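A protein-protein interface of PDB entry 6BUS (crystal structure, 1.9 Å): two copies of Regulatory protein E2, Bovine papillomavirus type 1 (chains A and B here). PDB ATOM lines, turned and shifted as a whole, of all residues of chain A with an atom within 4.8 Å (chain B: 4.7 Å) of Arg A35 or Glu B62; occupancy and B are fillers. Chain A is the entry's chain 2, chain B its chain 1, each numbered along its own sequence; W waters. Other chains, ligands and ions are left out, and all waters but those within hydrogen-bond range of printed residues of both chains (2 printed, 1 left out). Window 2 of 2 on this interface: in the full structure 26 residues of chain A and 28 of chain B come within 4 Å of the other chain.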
ATOM      1  N   VAL A  31      -4.306  21.196  -9.601  1.00  0.00           N
ATOM      2  CA  VAL A  31      -3.001  20.767 -10.058  1.00  0.00           C
ATOM      3  C   VAL A  31      -1.867  21.241  -9.141  1.00  0.00           C
ATOM      4  O   VAL A  31      -1.010  20.464  -8.787  1.00  0.00           O
ATOM      5  CB  VAL A  31      -2.817  21.220 -11.530  1.00  0.00           C
ATOM      6  CG1 VAL A  31      -1.401  21.042 -12.029  1.00  0.00           C
ATOM      7  CG2 VAL A  31      -3.740  20.413 -12.440  1.00  0.00           C
ATOM      8  N   LYS A  32      -1.850  22.529  -8.810  1.00  0.00           N
ATOM      9  CA  LYS A  32      -0.927  23.057  -7.851  1.00  0.00           C
ATOM     10  C   LYS A  32      -0.941  22.221  -6.564  1.00  0.00           C
ATOM     11  O   LYS A  32       0.072  21.856  -6.053  1.00  0.00           O
ATOM     12  CB  LYS A  32      -1.292  24.525  -7.567  1.00  0.00           C
ATOM     13  CG  LYS A  32      -0.799  25.101  -6.257  1.00  0.00           C
ATOM     14  CD  LYS A  32      -1.212  26.581  -6.100  1.00  0.00           C
ATOM     15  CE  LYS A  32      -0.072  27.306  -5.392  1.00  0.00           C
ATOM     16  NZ  LYS A  32      -0.327  28.715  -4.995  1.00  0.00           N
ATOM     17  N   CYS A  33      -2.127  21.917  -6.063  1.00  0.00           N
ATOM     18  CA  CYS A  33      -2.263  21.180  -4.802  1.00  0.00           C
ATOM     19  C   CYS A  33      -1.683  19.757  -4.932  1.00  0.00           C
ATOM     20  O   CYS A  33      -0.908  19.331  -4.112  1.00  0.00           O
ATOM     21  CB  CYS A  33      -3.705  21.156  -4.361  1.00  0.00           C
ATOM     22  SG  CYS A  33      -4.127  20.402  -2.739  1.00  0.00           S
ATOM     23  N   TYR A  34      -2.017  19.084  -6.013  1.00  0.00           N
ATOM     24  CA  TYR A  34      -1.522  17.748  -6.307  1.00  0.00           C
ATOM     25  C   TYR A  34       0.012  17.744  -6.381  1.00  0.00           C
ATOM     26  O   TYR A  34       0.670  16.875  -5.813  1.00  0.00           O
ATOM     27  CB  TYR A  34      -2.130  17.349  -7.648  1.00  0.00           C
ATOM     28  CG  TYR A  34      -1.832  15.957  -8.085  1.00  0.00           C
ATOM     29  CD1 TYR A  34      -0.552  15.587  -8.607  1.00  0.00           C
ATOM     30  CD2 TYR A  34      -2.793  14.996  -7.971  1.00  0.00           C
ATOM     31  CE1 TYR A  34      -0.312  14.259  -8.989  1.00  0.00           C
ATOM     32  CE2 TYR A  34      -2.563  13.689  -8.368  1.00  0.00           C
ATOM     33  CZ  TYR A  34      -1.346  13.326  -8.894  1.00  0.00           C
ATOM     34  OH  TYR A  34      -1.251  12.032  -9.288  1.00  0.00           O
ATOM     35  N   ARG A  35       0.585  18.743  -7.070  1.00  0.00           N
ATOM     36  CA  ARG A  35       2.040  18.844  -7.192  1.00  0.00           C
ATOM     37  C   ARG A  35       2.686  19.017  -5.818  1.00  0.00           C
ATOM     38  O   ARG A  35       3.663  18.364  -5.520  1.00  0.00           O
ATOM     39  CB  ARG A  35       2.459  20.007  -8.119  1.00  0.00           C
ATOM     40  CG  ARG A  35       3.979  20.068  -8.357  1.00  0.00           C
ATOM     41  CD  ARG A  35       4.391  21.075  -9.442  1.00  0.00           C
ATOM     42  NE  ARG A  35       3.825  22.416  -9.245  1.00  0.00           N
ATOM     43  CZ  ARG A  35       2.933  23.013 -10.021  1.00  0.00           C
ATOM     44  NH1 ARG A  35       2.505  22.461 -11.150  1.00  0.00           N
ATOM     45  NH2 ARG A  35       2.474  24.214  -9.666  1.00  0.00           N
ATOM     46  N   PHE A  36       2.137  19.909  -4.983  1.00  0.00           N
ATOM     47  CA  PHE A  36       2.686  20.111  -3.623  1.00  0.00           C
ATOM     48  C   PHE A  36       2.581  18.818  -2.821  1.00  0.00           C
ATOM     49  O   PHE A  36       3.530  18.419  -2.112  1.00  0.00           O
ATOM     50  CB  PHE A  36       1.940  21.275  -2.919  1.00  0.00           C
ATOM     51  CG  PHE A  36       2.178  21.378  -1.426  1.00  0.00           C
ATOM     52  CD1 PHE A  36       1.346  20.695  -0.515  1.00  0.00           C
ATOM     53  CD2 PHE A  36       3.157  22.217  -0.910  1.00  0.00           C
ATOM     54  CE1 PHE A  36       1.537  20.803   0.871  1.00  0.00           C
ATOM     55  CE2 PHE A  36       3.361  22.319   0.493  1.00  0.00           C
ATOM     56  CZ  PHE A  36       2.569  21.598   1.372  1.00  0.00           C
ATOM     57  N   ARG A  37       1.449  18.145  -2.933  1.00  0.00           N
ATOM     58  CA  ARG A  37       1.321  16.902  -2.184  1.00  0.00           C
ATOM     59  C   ARG A  37       2.348  15.834  -2.548  1.00  0.00           C
ATOM     60  O   ARG A  37       2.888  15.145  -1.649  1.00  0.00           O
ATOM     61  CB  ARG A  37      -0.099  16.331  -2.234  1.00  0.00           C
ATOM     62  CG  ARG A  37      -1.047  17.108  -1.353  1.00  0.00           C
ATOM     63  CD  ARG A  37      -2.459  16.603  -1.563  1.00  0.00           C
ATOM     64  NE  ARG A  37      -3.421  17.201  -0.602  1.00  0.00           N
ATOM     65  CZ  ARG A  37      -4.763  17.191  -0.751  1.00  0.00           C
ATOM     66  NH1 ARG A  37      -5.367  16.701  -1.853  1.00  0.00           N
ATOM     67  NH2 ARG A  37      -5.525  17.743   0.180  1.00  0.00           N
ATOM     68  N   VAL A  38       2.574  15.647  -3.846  1.00  0.00           N
ATOM     69  CA  VAL A  38       3.467  14.565  -4.246  1.00  0.00           C
ATOM     70  C   VAL A  38       4.921  14.929  -3.972  1.00  0.00           C
ATOM     71  O   VAL A  38       5.719  14.054  -3.601  1.00  0.00           O
ATOM     72  CB  VAL A  38       3.276  14.085  -5.716  1.00  0.00           C
ATOM     73  CG1 VAL A  38       1.892  13.533  -5.954  1.00  0.00           C
ATOM     74  CG2 VAL A  38       3.595  15.174  -6.723  1.00  0.00           C
ATOM     75  N   LYS A  39       5.263  16.218  -4.138  1.00  0.00           N
ATOM     76  CA  LYS A  39       6.584  16.708  -3.803  1.00  0.00           C
ATOM     77  C   LYS A  39       6.890  16.447  -2.358  1.00  0.00           C
ATOM     78  O   LYS A  39       8.031  16.052  -2.025  1.00  0.00           O
ATOM     79  CB  LYS A  39       6.729  18.206  -4.030  1.00  0.00           C
ATOM     80  CG  LYS A  39       8.168  18.730  -3.938  1.00  0.00           C
ATOM     81  CD  LYS A  39       8.199  20.245  -4.192  1.00  0.00           C
ATOM     82  CE  LYS A  39       8.123  20.618  -5.695  1.00  0.00           C
ATOM     83  NZ  LYS A  39       8.154  22.084  -6.029  1.00  0.00           N
ATOM     84  N   CYS A  49       8.447  16.584 -12.074  1.00  0.00           N
ATOM     85  CA  CYS A  49       7.181  17.152 -12.382  1.00  0.00           C
ATOM     86  C   CYS A  49       7.383  18.520 -13.072  1.00  0.00           C
ATOM     87  O   CYS A  49       8.315  19.249 -12.802  1.00  0.00           O
ATOM     88  CB  CYS A  49       6.417  17.372 -11.054  1.00  0.00           C
ATOM     89  SG  CYS A  49       4.661  17.809 -11.250  1.00  0.00           S
ATOM     90  N   THR A  50       6.468  18.907 -13.938  1.00  0.00           N
ATOM     91  CA  THR A  50       6.509  20.260 -14.469  1.00  0.00           C
ATOM     92  C   THR A  50       5.754  21.280 -13.625  1.00  0.00           C
ATOM     93  O   THR A  50       4.889  20.947 -12.799  1.00  0.00           O
ATOM     94  CB  THR A  50       5.868  20.288 -15.870  1.00  0.00           C
ATOM     95  OG1 THR A  50       4.473  19.973 -15.822  1.00  0.00           O
ATOM     96  CG2 THR A  50       6.553  19.307 -16.772  1.00  0.00           C
ATOM     97  N   THR A  51       6.047  22.545 -13.866  1.00  0.00           N
ATOM     98  CA  THR A  51       5.144  23.609 -13.453  1.00  0.00           C
ATOM     99  C   THR A  51       3.862  23.441 -14.267  1.00  0.00           C
ATOM    100  O   THR A  51       3.800  22.624 -15.169  1.00  0.00           O
ATOM    101  CB  THR A  51       5.782  24.996 -13.679  1.00  0.00           C
ATOM    102  OG1 THR A  51       6.282  25.118 -15.020  1.00  0.00           O
ATOM    103  CG2 THR A  51       6.893  25.179 -12.737  1.00  0.00           C
ATOM    104  N   THR A  52       2.831  24.176 -13.896  1.00  0.00           N
ATOM    105  CA  THR A  52       1.563  24.051 -14.513  1.00  0.00           C
ATOM    106  C   THR A  52       1.525  24.673 -15.905  1.00  0.00           C
ATOM    107  O   THR A  52       2.082  25.690 -16.120  1.00  0.00           O
ATOM    108  CB  THR A  52       0.546  24.742 -13.613  1.00  0.00           C
ATOM    109  OG1 THR A  52       0.581  24.120 -12.334  1.00  0.00           O
ATOM    110  CG2 THR A  52      -0.887  24.694 -14.197  1.00  0.00           C
ATOM    111  N   ILE A  69      -0.054  19.119 -15.833  1.00  0.00           N
ATOM    112  CA  ILE A  69       1.332  18.917 -15.414  1.00  0.00           C
ATOM    113  C   ILE A  69       1.730  17.593 -15.995  1.00  0.00           C
ATOM    114  O   ILE A  69       0.866  16.717 -16.180  1.00  0.00           O
ATOM    115  CB  ILE A  69       1.562  18.866 -13.869  1.00  0.00           C
ATOM    116  CG1 ILE A  69       0.632  17.877 -13.162  1.00  0.00           C
ATOM    117  CG2 ILE A  69       1.459  20.283 -13.248  1.00  0.00           C
ATOM    118  CD1 ILE A  69       0.916  17.649 -11.677  1.00  0.00           C
ATOM    119  N   THR B  55      10.796  22.446 -15.554  1.00  0.00           N
ATOM    120  CA  THR B  55      10.953  21.330 -14.679  1.00  0.00           C
ATOM    121  C   THR B  55      10.968  21.945 -13.264  1.00  0.00           C
ATOM    122  O   THR B  55      11.756  22.873 -12.944  1.00  0.00           O
ATOM    123  CB  THR B  55      12.242  20.562 -14.930  1.00  0.00           C
ATOM    124  OG1 THR B  55      12.228  20.053 -16.261  1.00  0.00           O
ATOM    125  CG2 THR B  55      12.402  19.409 -13.959  1.00  0.00           C
ATOM    126  N   VAL B  56      10.035  21.470 -12.464  1.00  0.00           N
ATOM    127  CA  VAL B  56       9.795  22.047 -11.161  1.00  0.00           C
ATOM    128  C   VAL B  56      10.922  21.737 -10.185  1.00  0.00           C
ATOM    129  O   VAL B  56      11.346  20.575 -10.062  1.00  0.00           O
ATOM    130  CB  VAL B  56       8.421  21.587 -10.634  1.00  0.00           C
ATOM    131  CG1 VAL B  56       8.463  20.232  -9.923  1.00  0.00           C
ATOM    132  CG2 VAL B  56       7.850  22.606  -9.676  1.00  0.00           C
ATOM    133  N   ALA B  57      11.433  22.773  -9.515  1.00  0.00           N
ATOM    134  CA  ALA B  57      12.397  22.577  -8.416  1.00  0.00           C
ATOM    135  C   ALA B  57      11.710  22.280  -7.065  1.00  0.00           C
ATOM    136  O   ALA B  57      10.567  22.685  -6.821  1.00  0.00           O
ATOM    137  CB  ALA B  57      13.298  23.772  -8.322  1.00  0.00           C
ATOM    138  N   GLY B  60      12.675  26.592  -3.072  1.00  0.00           N
ATOM    139  CA  GLY B  60      12.843  27.920  -3.626  1.00  0.00           C
ATOM    140  C   GLY B  60      11.782  28.181  -4.635  1.00  0.00           C
ATOM    141  O   GLY B  60      10.684  27.699  -4.476  1.00  0.00           O
ATOM    142  N   ALA B  61      12.095  28.962  -5.656  1.00  0.00           N
ATOM    143  CA  ALA B  61      11.108  29.257  -6.677  1.00  0.00           C
ATOM    144  C   ALA B  61      10.934  27.981  -7.522  1.00  0.00           C
ATOM    145  O   ALA B  61      11.928  27.428  -7.913  1.00  0.00           O
ATOM    146  CB  ALA B  61      11.580  30.406  -7.528  1.00  0.00           C
ATOM    147  N   GLU B  62       9.711  27.506  -7.780  1.00  0.00           N
ATOM    148  CA  GLU B  62       9.563  26.280  -8.622  1.00  0.00           C
ATOM    149  C   GLU B  62      10.171  26.466 -10.021  1.00  0.00           C
ATOM    150  O   GLU B  62      10.884  25.588 -10.494  1.00  0.00           O
ATOM    151  CB  GLU B  62       8.119  25.841  -8.765  1.00  0.00           C
ATOM    152  CG  GLU B  62       7.593  25.106  -7.553  1.00  0.00           C
ATOM    153  CD  GLU B  62       6.163  24.609  -7.733  1.00  0.00           C
ATOM    154  OE1 GLU B  62       5.298  25.399  -8.123  1.00  0.00           O
ATOM    155  OE2 GLU B  62       5.890  23.423  -7.455  1.00  0.00           O
ATOM    156  N   ARG B  63       9.952  27.636 -10.619  1.00  0.00           N
ATOM    157  CA  ARG B  63      10.388  27.903 -12.009  1.00  0.00           C
ATOM    158  C   ARG B  63      11.904  27.941 -12.098  1.00  0.00           C
ATOM    159  O   ARG B  63      12.507  28.924 -11.688  1.00  0.00           O
ATOM    160  CB  ARG B  63       9.732  29.191 -12.568  1.00  0.00           C
ATOM    161  CG  ARG B  63       8.226  29.255 -12.294  1.00  0.00           C
ATOM    162  CD  ARG B  63       7.358  29.963 -13.322  1.00  0.00           C
ATOM    163  NE  ARG B  63       5.974  30.110 -12.809  1.00  0.00           N
ATOM    164  CZ  ARG B  63       4.917  29.332 -13.106  1.00  0.00           C
ATOM    165  NH1 ARG B  63       5.015  28.311 -13.960  1.00  0.00           N
ATOM    166  NH2 ARG B  63       3.720  29.591 -12.557  1.00  0.00           N
ATOM    167  N   GLN B  64      12.518  26.880 -12.600  1.00  0.00           N
ATOM    168  CA  GLN B  64      13.988  26.778 -12.758  1.00  0.00           C
ATOM    169  C   GLN B  64      14.478  26.056 -14.051  1.00  0.00           C
ATOM    170  O   GLN B  64      13.737  25.295 -14.656  1.00  0.00           O
ATOM    171  CB  GLN B  64      14.644  26.133 -11.520  1.00  0.00           C
ATOM    172  CG  GLN B  64      14.328  26.740 -10.151  1.00  0.00           C
ATOM    173  CD  GLN B  64      14.939  28.121  -9.881  1.00  0.00           C
ATOM    174  OE1 GLN B  64      14.439  28.841  -9.065  1.00  0.00           O
ATOM    175  NE2 GLN B  64      15.972  28.488 -10.596  1.00  0.00           N
HETATM  176  O   HOH W   1       4.367  26.749 -16.315  1.00  0.00           O
HETATM  177  O   HOH W   2      10.777  18.052 -10.439  1.00  0.00           O
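The backbone NH (N) of Val B56 sits at hydrogen-bond distance from the backbone carbonyl oxygen (O) of Cys A49 (2.8 Å).
NZ of Lys A39 sits at hydrogen-bond distance from O of Ala B57 (2.6 Å).
NE of Arg A35 is in salt-bridge range of OE2 of Glu B62 (2.9 Å).
NZ of Lys A39 is in salt-bridge range of OE2 of Glu B62 (3.0 Å).
O of Glu B62 sits at hydrogen-bond distance from N of Ala B57 (3.0 Å).
NH1 of Arg A35 is in hydrogen-bond range of O of Thr A50.
The side-chain hydroxyl of Thr A52 sits at hydrogen-bond distance from the guanidinium group of Arg A35 (2.8 Å).
Among the printed residues, pairs that only touch across the chains: Arg A35 with Val B56 (3.8 Å), Lys A39 with Val B56 (3.7 Å), Cys A49 with Thr B55 (3.8 Å) and Thr A51 with Arg B63 (3.4 Å).
Val A31 touches none of the printed residues of chain B.
Of the printed residues of chain B, Arg A35 touches Val B56 (3.8 Å) and Glu B62 (2.9 Å).
Of the printed residues of chain B, Cys A49 touches Thr B55 (3.8 Å) and Val B56 (2.8 Å).
Printed residues of chain A within 4 Å of Thr B55: Cys A49.
Printed residues of chain A within 4 Å of Ala B57: Lys A39.
Glu B62 touches just these residues of chain A: Arg A35 (2.9 Å) and Lys A39 (3.0 Å).
Printed residues of chain A within 4 Å of Arg B63: Thr A51.
Gln B64 touches none of the printed residues of chain A.
The nearest printed residue of chain B that does not touch Arg A35 is Arg B63 (6.2 Å).
The nearest residue of chain A that does not touch Glu B62 is Thr A51 (4.2 Å).
Of the 14 printed residues of chain A, 4 touch a printed residue of chain B.
Printed residues of chain A that touch a printed residue of chain B: Arg A35, Lys A39, Cys A49 and Thr A51.
Hydrophobic or aromatic side chains of chain B that line the printed part of chain A: Val B56.
Among the printed residues, 8 pairs touch across the chains.
Among the printed residues, Asp or Glu carboxylates within 4 Å of a Lys or Arg side-chain nitrogen of the other chain: Arg A35 with Glu B62 and Lys A39 with Glu B62.
No position is printed for both chains.
Water W1 lies within hydrogen-bond range of the backbone carbonyl oxygen (O) of Thr A52 (2.5 Å), the side-chain hydroxyl (OG1) of Thr A51 (2.8 Å) and the guanidinium group (NH1) of Arg B63 (2.9 Å).
Water W2 bridges the backbone carbonyl oxygen (O) of Val B56 (2.6 Å) and the backbone NH (N) of Cys A49 (3.2 Å).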
